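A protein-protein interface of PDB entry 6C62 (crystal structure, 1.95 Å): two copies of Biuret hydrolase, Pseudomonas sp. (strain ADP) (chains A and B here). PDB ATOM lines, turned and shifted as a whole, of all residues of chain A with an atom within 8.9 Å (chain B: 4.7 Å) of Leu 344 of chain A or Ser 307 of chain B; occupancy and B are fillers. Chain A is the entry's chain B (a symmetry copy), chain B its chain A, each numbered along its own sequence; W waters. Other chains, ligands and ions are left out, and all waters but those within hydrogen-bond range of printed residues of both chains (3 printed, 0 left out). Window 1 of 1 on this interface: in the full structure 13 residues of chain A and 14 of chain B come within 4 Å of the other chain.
SG of Cys 311 of chain B lies within hydrogen-bond range of O of Ser 307 of chain B, 3.2 Å away.
The side-chain hydroxyl of Ser 307 of chain B lies within hydrogen-bond range of the backbone carbonyl oxygen of Gly 335 of chain B (2.9 Å).
The side-chain hydroxyl (OH) of Tyr 343 of chain A is in hydrogen-bond range of the side-chain amide nitrogen (NE2) of Gln 347 of chain A (2.9 Å).
OE2 of Glu 308 of chain B is in hydrogen-bond range of OH of Tyr 343 of chain B, at 2.6 Å.
NE2 of Gln 338 of chain B sits at hydrogen-bond distance from OG of Ser 307 of chain B, at 2.9 Å.
NE2 of Gln 338 of chain B sits at hydrogen-bond distance from O of Val 303 of chain B (3.1 Å).
CG1 of Val 340 of chain A touches OG of Ser 307 of chain B, 3.8 Å away.
SG of Cys 311 of chain B touches CG1 of Val 340 of chain A, at 3.9 Å.
Gln 338 of chain B touches Val 340 of chain A.
Tyr 343 of chain B touches Val 340 of chain A.
Cys 311 of chain B touches Ala 341 of chain A (SG to CA, 3.6 Å).
Tyr 343 of chain B touches Tyr 343 of chain A.
CD1 of Leu 344 of chain A touches O of Ser 307 of chain B, 3.6 Å away.
Cys 311 of chain B touches Leu 344 of chain A (CB to CD1, 3.8 Å).
Tyr 343 of chain B touches Leu 344 of chain A (OH to CD2, 3.6 Å).
Leu 312 of chain B touches Arg 348 of chain A.
Of chain A, only Val 340 (3.8 Å) and Leu 344 (3.6 Å) come within 4 Å of Ser 307 of chain B.
No residue of chain A comes within 4 Å of Ala 306 of chain B.
Of the printed residues of chain A, Tyr 343 of chain B touches Val 340, Tyr 343 and Leu 344.
Printed residues of chain B within 4 Å of Ala 341 of chain A: Cys 311.
Printed residues of chain B within 4 Å of Val 340 of chain A: Ser 307, Cys 311, Gln 338 and Tyr 343.
Of the printed residues of chain A, Leu 312 of chain B touches Arg 348 (3.8 Å).
Phe 349 of chain A touches none of the printed residues of chain B.
The nearest printed residue of chain B that does not touch Leu 344 of chain A is Glu 308 of chain B (4.004 Å).
The nearest residue of chain A that does not touch Ser 307 of chain B is Ala 341 of chain A (6.4 Å).
Of the 18 printed residues of chain A, 5 touch a printed residue of chain B.
Printed residues of chain A that touch a printed residue of chain B: Val 340, Ala 341, Tyr 343, Leu 344 and Arg 348.
Hydrophobic or aromatic side chains of chain A within 4 Å of the printed part of chain B: Val 340, Ala 341, Tyr 343 and Leu 344.
Printed residues of chain B that touch a printed residue of chain A: Ser 307, Cys 311, Leu 312, Gln 338 and Tyr 343.
Hydrophobic or aromatic side chains of chain B that line the printed part of chain A: Leu 312 and Tyr 343.
Among the printed residues, no Asp or Glu carboxylate lies within 4 Å of a Lys or Arg side-chain nitrogen of the other chain.
Tyr 343 of chain B touches its own counterpart, Tyr 343 of chain A.
5 positions are printed for both chains.
Of the 10 pairs that touch across the chains among the printed residues, 1 has its exchanged pair printed and touching as well.
Water W1 lies within hydrogen-bond range of O of Gln 338 of chain B (2.5 Å) and N of Val 340 of chain A (3.0 Å).
Water W2 lies within hydrogen-bond range of O of Cys 311 of chain B (2.7 Å), NH1 of Arg 348 of chain A (3.2 Å) and O of Leu 312 of chain B (3.3 Å).
Water W3 bridges NH2 of Arg 348 of chain A (2.9 Å) and O of Leu 312 of chain B (3.0 Å).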
ATOM      1  N   ALA A 300     -26.359  -5.787 -28.717  1.00  0.00           N
ATOM      2  CA  ALA A 300     -25.496  -5.761 -27.559  1.00  0.00           C
ATOM      3  C   ALA A 300     -25.088  -4.328 -27.188  1.00  0.00           C
ATOM      4  O   ALA A 300     -25.086  -3.975 -26.000  1.00  0.00           O
ATOM      5  CB  ALA A 300     -24.265  -6.606 -27.819  1.00  0.00           C
ATOM      6  N   VAL A 303     -28.152  -2.717 -25.497  1.00  0.00           N
ATOM      7  CA  VAL A 303     -28.287  -3.201 -24.138  1.00  0.00           C
ATOM      8  C   VAL A 303     -27.303  -2.550 -23.165  1.00  0.00           C
ATOM      9  O   VAL A 303     -27.678  -2.102 -22.091  1.00  0.00           O
ATOM     10  CB  VAL A 303     -28.235  -4.756 -24.124  1.00  0.00           C
ATOM     11  CG1 VAL A 303     -28.035  -5.283 -22.732  1.00  0.00           C
ATOM     12  CG2 VAL A 303     -29.559  -5.307 -24.681  1.00  0.00           C
ATOM     13  N   ILE A 304     -26.040  -2.543 -23.506  1.00  0.00           N
ATOM     14  CA  ILE A 304     -25.008  -1.966 -22.654  1.00  0.00           C
ATOM     15  C   ILE A 304     -25.213  -0.456 -22.473  1.00  0.00           C
ATOM     16  O   ILE A 304     -25.055   0.050 -21.394  1.00  0.00           O
ATOM     17  CB  ILE A 304     -23.637  -2.285 -23.237  1.00  0.00           C
ATOM     18  CG1 ILE A 304     -23.322  -3.753 -22.962  1.00  0.00           C
ATOM     19  CG2 ILE A 304     -22.526  -1.390 -22.657  1.00  0.00           C
ATOM     20  CD1 ILE A 304     -22.199  -4.308 -23.815  1.00  0.00           C
ATOM     21  N   SER A 307     -28.314   0.315 -20.023  1.00  0.00           N
ATOM     22  CA  SER A 307     -28.022   0.089 -18.600  1.00  0.00           C
ATOM     23  C   SER A 307     -26.954   1.020 -18.029  1.00  0.00           C
ATOM     24  O   SER A 307     -27.129   1.547 -16.929  1.00  0.00           O
ATOM     25  CB  SER A 307     -27.650  -1.376 -18.377  1.00  0.00           C
ATOM     26  OG  SER A 307     -28.863  -2.172 -18.458  1.00  0.00           O
ATOM     27  N   GLN A 338     -33.259  -3.155 -16.788  1.00  0.00           N
ATOM     28  CA  GLN A 338     -32.858  -4.305 -17.580  1.00  0.00           C
ATOM     29  C   GLN A 338     -32.213  -5.352 -16.714  1.00  0.00           C
ATOM     30  O   GLN A 338     -31.379  -5.035 -15.869  1.00  0.00           O
ATOM     31  CB  GLN A 338     -31.925  -3.914 -18.719  1.00  0.00           C
ATOM     32  CG  GLN A 338     -32.553  -3.141 -19.842  1.00  0.00           C
ATOM     33  CD  GLN A 338     -31.535  -2.620 -20.830  1.00  0.00           C
ATOM     34  OE1 GLN A 338     -31.913  -1.822 -21.677  1.00  0.00           O
ATOM     35  NE2 GLN A 338     -30.267  -3.078 -20.764  1.00  0.00           N
ATOM     36  N   PRO A 339     -32.648  -6.621 -16.861  1.00  0.00           N
ATOM     37  CA  PRO A 339     -31.969  -7.691 -16.125  1.00  0.00           C
ATOM     38  C   PRO A 339     -30.394  -7.619 -16.312  1.00  0.00           C
ATOM     39  O   PRO A 339     -29.872  -7.339 -17.411  1.00  0.00           O
ATOM     40  CB  PRO A 339     -32.535  -8.979 -16.810  1.00  0.00           C
ATOM     41  CG  PRO A 339     -33.903  -8.595 -17.252  1.00  0.00           C
ATOM     42  CD  PRO A 339     -33.821  -7.110 -17.621  1.00  0.00           C
ATOM     43  N   VAL A 340     -29.687  -7.898 -15.234  1.00  0.00           N
ATOM     44  CA  VAL A 340     -28.245  -8.017 -15.259  1.00  0.00           C
ATOM     45  C   VAL A 340     -27.815  -9.099 -16.251  1.00  0.00           C
ATOM     46  O   VAL A 340     -26.752  -8.988 -16.857  1.00  0.00           O
ATOM     47  CB  VAL A 340     -27.689  -8.231 -13.871  1.00  0.00           C
ATOM     48  CG1 VAL A 340     -28.012  -9.636 -13.347  1.00  0.00           C
ATOM     49  CG2 VAL A 340     -26.173  -8.007 -13.849  1.00  0.00           C
ATOM     50  N   ALA A 341     -28.607 -10.150 -16.450  1.00  0.00           N
ATOM     51  CA  ALA A 341     -28.189 -11.169 -17.409  1.00  0.00           C
ATOM     52  C   ALA A 341     -27.984 -10.630 -18.850  1.00  0.00           C
ATOM     53  O   ALA A 341     -27.079 -11.106 -19.594  1.00  0.00           O
ATOM     54  CB  ALA A 341     -29.177 -12.287 -17.415  1.00  0.00           C
ATOM     55  N   TRP A 342     -28.779  -9.634 -19.217  1.00  0.00           N
ATOM     56  CA  TRP A 342     -28.686  -9.058 -20.589  1.00  0.00           C
ATOM     57  C   TRP A 342     -27.366  -8.322 -20.713  1.00  0.00           C
ATOM     58  O   TRP A 342     -26.641  -8.500 -21.730  1.00  0.00           O
ATOM     59  CB  TRP A 342     -29.794  -8.083 -20.878  1.00  0.00           C
ATOM     60  CG  TRP A 342     -31.185  -8.655 -20.818  1.00  0.00           C
ATOM     61  CD1 TRP A 342     -31.525  -9.934 -20.682  1.00  0.00           C
ATOM     62  CD2 TRP A 342     -32.398  -7.934 -21.023  1.00  0.00           C
ATOM     63  NE1 TRP A 342     -32.904 -10.067 -20.736  1.00  0.00           N
ATOM     64  CE2 TRP A 342     -33.446  -8.840 -20.933  1.00  0.00           C
ATOM     65  CE3 TRP A 342     -32.686  -6.592 -21.338  1.00  0.00           C
ATOM     66  CZ2 TRP A 342     -34.790  -8.470 -21.117  1.00  0.00           C
ATOM     67  CZ3 TRP A 342     -34.018  -6.204 -21.502  1.00  0.00           C
ATOM     68  CH2 TRP A 342     -35.053  -7.128 -21.390  1.00  0.00           C
ATOM     69  N   TYR A 343     -27.018  -7.567 -19.664  1.00  0.00           N
ATOM     70  CA  TYR A 343     -25.762  -6.807 -19.652  1.00  0.00           C
ATOM     71  C   TYR A 343     -24.553  -7.755 -19.770  1.00  0.00           C
ATOM     72  O   TYR A 343     -23.616  -7.551 -20.563  1.00  0.00           O
ATOM     73  CB  TYR A 343     -25.660  -5.926 -18.408  1.00  0.00           C
ATOM     74  CG  TYR A 343     -24.401  -5.122 -18.351  1.00  0.00           C
ATOM     75  CD1 TYR A 343     -24.300  -3.928 -19.058  1.00  0.00           C
ATOM     76  CD2 TYR A 343     -23.276  -5.580 -17.692  1.00  0.00           C
ATOM     77  CE1 TYR A 343     -23.132  -3.189 -19.101  1.00  0.00           C
ATOM     78  CE2 TYR A 343     -22.067  -4.825 -17.689  1.00  0.00           C
ATOM     79  CZ  TYR A 343     -22.024  -3.600 -18.394  1.00  0.00           C
ATOM     80  OH  TYR A 343     -20.906  -2.852 -18.403  1.00  0.00           O
ATOM     81  N   LEU A 344     -24.525  -8.758 -18.906  1.00  0.00           N
ATOM     82  CA  LEU A 344     -23.390  -9.698 -18.875  1.00  0.00           C
ATOM     83  C   LEU A 344     -23.232 -10.484 -20.192  1.00  0.00           C
ATOM     84  O   LEU A 344     -22.132 -10.649 -20.714  1.00  0.00           O
ATOM     85  CB  LEU A 344     -23.534 -10.633 -17.690  1.00  0.00           C
ATOM     86  CG  LEU A 344     -23.310  -9.949 -16.344  1.00  0.00           C
ATOM     87  CD1 LEU A 344     -23.788 -10.859 -15.231  1.00  0.00           C
ATOM     88  CD2 LEU A 344     -21.882  -9.455 -16.201  1.00  0.00           C
ATOM     89  N   ARG A 345     -24.362 -10.924 -20.718  1.00  0.00           N
ATOM     90  CA  ARG A 345     -24.341 -11.562 -22.022  1.00  0.00           C
ATOM     91  C   ARG A 345     -23.791 -10.712 -23.143  1.00  0.00           C
ATOM     92  O   ARG A 345     -22.976 -11.168 -23.954  1.00  0.00           O
ATOM     93  CB  ARG A 345     -25.712 -12.133 -22.362  1.00  0.00           C
ATOM     94  CG  ARG A 345     -25.577 -12.991 -23.606  1.00  0.00           C
ATOM     95  CD  ARG A 345     -26.848 -13.750 -23.901  1.00  0.00           C
ATOM     96  NE  ARG A 345     -26.641 -15.066 -23.436  1.00  0.00           N
ATOM     97  CZ  ARG A 345     -26.124 -16.080 -24.099  1.00  0.00           C
ATOM     98  NH1 ARG A 345     -25.857 -17.143 -23.420  1.00  0.00           N
ATOM     99  NH2 ARG A 345     -25.819 -16.047 -25.335  1.00  0.00           N
ATOM    100  N   ALA A 346     -24.204  -9.432 -23.161  1.00  0.00           N
ATOM    101  CA  ALA A 346     -23.669  -8.477 -24.104  1.00  0.00           C
ATOM    102  C   ALA A 346     -22.171  -8.223 -23.974  1.00  0.00           C
ATOM    103  O   ALA A 346     -21.451  -8.147 -24.995  1.00  0.00           O
ATOM    104  CB  ALA A 346     -24.457  -7.181 -24.007  1.00  0.00           C
ATOM    105  N   GLN A 347     -21.675  -8.162 -22.765  1.00  0.00           N
ATOM    106  CA  GLN A 347     -20.243  -8.010 -22.510  1.00  0.00           C
ATOM    107  C   GLN A 347     -19.436  -9.273 -22.927  1.00  0.00           C
ATOM    108  O   GLN A 347     -18.274  -9.144 -23.418  1.00  0.00           O
ATOM    109  CB  GLN A 347     -19.967  -7.652 -21.069  1.00  0.00           C
ATOM    110  CG  GLN A 347     -20.334  -6.224 -20.634  1.00  0.00           C
ATOM    111  CD  GLN A 347     -19.421  -5.140 -21.244  1.00  0.00           C
ATOM    112  OE1 GLN A 347     -18.557  -5.442 -22.069  1.00  0.00           O
ATOM    113  NE2 GLN A 347     -19.647  -3.836 -20.869  1.00  0.00           N
ATOM    114  N   ARG A 348     -20.036 -10.456 -22.776  1.00  0.00           N
ATOM    115  CA  ARG A 348     -19.395 -11.680 -23.181  1.00  0.00           C
ATOM    116  C   ARG A 348     -19.422 -11.797 -24.698  1.00  0.00           C
ATOM    117  O   ARG A 348     -18.421 -12.189 -25.319  1.00  0.00           O
ATOM    118  CB  ARG A 348     -20.037 -12.910 -22.524  1.00  0.00           C
ATOM    119  CG  ARG A 348     -19.743 -12.929 -21.031  1.00  0.00           C
ATOM    120  CD  ARG A 348     -20.569 -13.963 -20.243  1.00  0.00           C
ATOM    121  NE  ARG A 348     -20.223 -15.312 -20.626  1.00  0.00           N
ATOM    122  CZ  ARG A 348     -21.044 -16.360 -20.599  1.00  0.00           C
ATOM    123  NH1 ARG A 348     -22.289 -16.272 -20.188  1.00  0.00           N
ATOM    124  NH2 ARG A 348     -20.606 -17.532 -21.023  1.00  0.00           N
ATOM    125  N   PHE A 349     -20.557 -11.440 -25.298  1.00  0.00           N
ATOM    126  CA  PHE A 349     -20.661 -11.411 -26.743  1.00  0.00           C
ATOM    127  C   PHE A 349     -19.663 -10.414 -27.337  1.00  0.00           C
ATOM    128  O   PHE A 349     -19.091 -10.654 -28.393  1.00  0.00           O
ATOM    129  CB  PHE A 349     -22.076 -11.063 -27.179  1.00  0.00           C
ATOM    130  CG  PHE A 349     -22.177 -10.785 -28.659  1.00  0.00           C
ATOM    131  CD1 PHE A 349     -22.091 -11.829 -29.579  1.00  0.00           C
ATOM    132  CD2 PHE A 349     -22.315  -9.535 -29.108  1.00  0.00           C
ATOM    133  CE1 PHE A 349     -22.128 -11.574 -30.955  1.00  0.00           C
ATOM    134  CE2 PHE A 349     -22.308  -9.264 -30.471  1.00  0.00           C
ATOM    135  CZ  PHE A 349     -22.238 -10.272 -31.375  1.00  0.00           C
ATOM    136  N   ARG A 350     -19.421  -9.284 -26.658  1.00  0.00           N
ATOM    137  CA  ARG A 350     -18.504  -8.302 -27.199  1.00  0.00           C
ATOM    138  C   ARG A 350     -17.083  -8.851 -27.435  1.00  0.00           C
ATOM    139  O   ARG A 350     -16.421  -8.413 -28.371  1.00  0.00           O
ATOM    140  CB  ARG A 350     -18.429  -7.041 -26.284  1.00  0.00           C
ATOM    141  CG  ARG A 350     -17.785  -5.856 -26.963  1.00  0.00           C
ATOM    142  CD  ARG A 350     -17.798  -4.623 -26.080  1.00  0.00           C
ATOM    143  NE  ARG A 350     -17.640  -3.409 -26.879  1.00  0.00           N
ATOM    144  CZ  ARG A 350     -17.509  -2.183 -26.336  1.00  0.00           C
ATOM    145  NH1 ARG A 350     -17.517  -2.028 -25.033  1.00  0.00           N
ATOM    146  NH2 ARG A 350     -17.397  -1.114 -27.129  1.00  0.00           N
ATOM    147  N   ARG A 351     -16.609  -9.773 -26.596  1.00  0.00           N
ATOM    148  CA  ARG A 351     -15.312 -10.479 -26.852  1.00  0.00           C
ATOM    149  C   ARG A 351     -15.371 -11.267 -28.166  1.00  0.00           C
ATOM    150  O   ARG A 351     -14.462 -11.167 -28.995  1.00  0.00           O
ATOM    151  CB  ARG A 351     -14.922 -11.363 -25.696  1.00  0.00           C
ATOM    152  CG  ARG A 351     -13.758 -12.327 -25.992  1.00  0.00           C
ATOM    153  CD  ARG A 351     -13.242 -13.080 -24.765  1.00  0.00           C
ATOM    154  NE  ARG A 351     -12.779 -12.136 -23.738  1.00  0.00           N
ATOM    155  CZ  ARG A 351     -11.559 -11.589 -23.701  1.00  0.00           C
ATOM    156  NH1 ARG A 351     -10.647 -11.888 -24.566  1.00  0.00           N
ATOM    157  NH2 ARG A 351     -11.256 -10.746 -22.734  1.00  0.00           N
ATOM    158  N   VAL B 303     -21.680  -9.023  -4.623  1.00  0.00           N
ATOM    159  CA  VAL B 303     -22.591  -8.628  -5.686  1.00  0.00           C
ATOM    160  C   VAL B 303     -22.150  -9.118  -7.043  1.00  0.00           C
ATOM    161  O   VAL B 303     -22.956  -9.701  -7.764  1.00  0.00           O
ATOM    162  CB  VAL B 303     -22.836  -7.073  -5.635  1.00  0.00           C
ATOM    163  CG1 VAL B 303     -23.505  -6.587  -6.897  1.00  0.00           C
ATOM    164  CG2 VAL B 303     -23.730  -6.719  -4.448  1.00  0.00           C
ATOM    165  N   ILE B 304     -20.918  -8.894  -7.391  1.00  0.00           N
ATOM    166  CA  ILE B 304     -20.370  -9.308  -8.687  1.00  0.00           C
ATOM    167  C   ILE B 304     -20.356 -10.830  -8.821  1.00  0.00           C
ATOM    168  O   ILE B 304     -20.655 -11.358  -9.830  1.00  0.00           O
ATOM    169  CB  ILE B 304     -18.963  -8.711  -8.854  1.00  0.00           C
ATOM    170  CG1 ILE B 304     -19.135  -7.211  -9.149  1.00  0.00           C
ATOM    171  CG2 ILE B 304     -18.150  -9.350  -9.972  1.00  0.00           C
ATOM    172  CD1 ILE B 304     -17.868  -6.378  -8.977  1.00  0.00           C
ATOM    173  N   THR B 305     -20.011 -11.501  -7.749  1.00  0.00           N
ATOM    174  CA  THR B 305     -19.932 -12.964  -7.706  1.00  0.00           C
ATOM    175  C   THR B 305     -21.292 -13.567  -8.014  1.00  0.00           C
ATOM    176  O   THR B 305     -21.392 -14.455  -8.841  1.00  0.00           O
ATOM    177  CB  THR B 305     -19.422 -13.445  -6.337  1.00  0.00           C
ATOM    178  OG1 THR B 305     -18.016 -13.109  -6.229  1.00  0.00           O
ATOM    179  CG2 THR B 305     -19.626 -14.919  -6.168  1.00  0.00           C
ATOM    180  N   ALA B 306     -22.314 -13.103  -7.303  1.00  0.00           N
ATOM    181  CA  ALA B 306     -23.628 -13.702  -7.446  1.00  0.00           C
ATOM    182  C   ALA B 306     -24.194 -13.494  -8.858  1.00  0.00           C
ATOM    183  O   ALA B 306     -24.778 -14.374  -9.408  1.00  0.00           O
ATOM    184  CB  ALA B 306     -24.583 -13.141  -6.409  1.00  0.00           C
ATOM    185  N   SER B 307     -24.075 -12.281  -9.393  1.00  0.00           N
ATOM    186  CA  SER B 307     -24.596 -12.042 -10.735  1.00  0.00           C
ATOM    187  C   SER B 307     -23.787 -12.764 -11.836  1.00  0.00           C
ATOM    188  O   SER B 307     -24.408 -13.352 -12.740  1.00  0.00           O
ATOM    189  CB  SER B 307     -24.683 -10.552 -10.997  1.00  0.00           C
ATOM    190  OG  SER B 307     -25.797 -10.078 -10.264  1.00  0.00           O
ATOM    191  N   GLU B 308     -22.468 -12.661 -11.795  1.00  0.00           N
ATOM    192  CA  GLU B 308     -21.671 -13.275 -12.841  1.00  0.00           C
ATOM    193  C   GLU B 308     -21.776 -14.833 -12.736  1.00  0.00           C
ATOM    194  O   GLU B 308     -21.945 -15.470 -13.727  1.00  0.00           O
ATOM    195  CB  GLU B 308     -20.198 -12.878 -12.767  1.00  0.00           C
ATOM    196  CG  GLU B 308     -19.895 -11.512 -13.276  1.00  0.00           C
ATOM    197  CD  GLU B 308     -18.390 -11.151 -13.445  1.00  0.00           C
ATOM    198  OE1 GLU B 308     -17.510 -12.031 -13.589  1.00  0.00           O
ATOM    199  OE2 GLU B 308     -18.075  -9.902 -13.490  1.00  0.00           O
ATOM    200  N   GLY B 309     -21.699 -15.410 -11.514  1.00  0.00           N
ATOM    201  CA  GLY B 309     -21.846 -16.876 -11.388  1.00  0.00           C
ATOM    202  C   GLY B 309     -23.258 -17.356 -11.727  1.00  0.00           C
ATOM    203  O   GLY B 309     -23.430 -18.330 -12.436  1.00  0.00           O
ATOM    204  N   GLY B 310     -24.282 -16.665 -11.245  1.00  0.00           N
ATOM    205  CA  GLY B 310     -25.648 -17.034 -11.590  1.00  0.00           C
ATOM    206  C   GLY B 310     -25.932 -16.943 -13.066  1.00  0.00           C
ATOM    207  O   GLY B 310     -26.519 -17.895 -13.656  1.00  0.00           O
ATOM    208  N   CYS B 311     -25.572 -15.817 -13.699  1.00  0.00           N
ATOM    209  CA  CYS B 311     -25.858 -15.635 -15.116  1.00  0.00           C
ATOM    210  C   CYS B 311     -25.094 -16.600 -15.990  1.00  0.00           C
ATOM    211  O   CYS B 311     -25.561 -16.989 -17.030  1.00  0.00           O
ATOM    212  CB  CYS B 311     -25.661 -14.192 -15.551  1.00  0.00           C
ATOM    213  SG  CYS B 311     -26.924 -13.159 -14.690  1.00  0.00           S
ATOM    214  N   LEU B 312     -23.911 -17.003 -15.575  1.00  0.00           N
ATOM    215  CA  LEU B 312     -23.167 -18.025 -16.285  1.00  0.00           C
ATOM    216  C   LEU B 312     -23.980 -19.307 -16.472  1.00  0.00           C
ATOM    217  O   LEU B 312     -23.753 -20.012 -17.427  1.00  0.00           O
ATOM    218  CB  LEU B 312     -21.919 -18.415 -15.523  1.00  0.00           C
ATOM    219  CG  LEU B 312     -20.772 -19.109 -16.271  1.00  0.00           C
ATOM    220  CD1 LEU B 312     -20.154 -18.139 -17.256  1.00  0.00           C
ATOM    221  CD2 LEU B 312     -19.727 -19.540 -15.244  1.00  0.00           C
ATOM    222  N   GLY B 335     -28.765 -14.265  -7.403  1.00  0.00           N
ATOM    223  CA  GLY B 335     -27.744 -13.540  -8.203  1.00  0.00           C
ATOM    224  C   GLY B 335     -28.258 -13.084  -9.560  1.00  0.00           C
ATOM    225  O   GLY B 335     -28.011 -11.942  -9.980  1.00  0.00           O
ATOM    226  N   GLN B 338     -30.571  -9.894  -9.428  1.00  0.00           N
ATOM    227  CA  GLN B 338     -30.036  -8.665  -8.856  1.00  0.00           C
ATOM    228  C   GLN B 338     -30.161  -7.525  -9.867  1.00  0.00           C
ATOM    229  O   GLN B 338     -29.855  -7.688 -11.052  1.00  0.00           O
ATOM    230  CB  GLN B 338     -28.558  -8.810  -8.441  1.00  0.00           C
ATOM    231  CG  GLN B 338     -28.366  -9.654  -7.215  1.00  0.00           C
ATOM    232  CD  GLN B 338     -26.944  -9.967  -6.879  1.00  0.00           C
ATOM    233  OE1 GLN B 338     -26.698 -10.774  -6.002  1.00  0.00           O
ATOM    234  NE2 GLN B 338     -25.990  -9.296  -7.526  1.00  0.00           N
ATOM    235  N   TYR B 343     -24.694  -4.259  -9.879  1.00  0.00           N
ATOM    236  CA  TYR B 343     -23.472  -4.765 -10.575  1.00  0.00           C
ATOM    237  C   TYR B 343     -22.592  -3.603 -11.046  1.00  0.00           C
ATOM    238  O   TYR B 343     -21.364  -3.588 -10.870  1.00  0.00           O
ATOM    239  CB  TYR B 343     -23.881  -5.676 -11.724  1.00  0.00           C
ATOM    240  CG  TYR B 343     -22.697  -6.249 -12.464  1.00  0.00           C
ATOM    241  CD1 TYR B 343     -22.044  -7.386 -11.973  1.00  0.00           C
ATOM    242  CD2 TYR B 343     -22.137  -5.594 -13.588  1.00  0.00           C
ATOM    243  CE1 TYR B 343     -20.891  -7.871 -12.575  1.00  0.00           C
ATOM    244  CE2 TYR B 343     -21.020  -6.115 -14.214  1.00  0.00           C
ATOM    245  CZ  TYR B 343     -20.408  -7.260 -13.718  1.00  0.00           C
ATOM    246  OH  TYR B 343     -19.294  -7.799 -14.335  1.00  0.00           O
HETATM  247  O   HOH W   1     -31.291  -8.715 -12.866  1.00  0.00           O
HETATM  248  O   HOH W   2     -25.040 -17.799 -19.582  1.00  0.00           O
HETATM  249  O   HOH W   3     -22.423 -19.634 -20.072  1.00  0.00           O
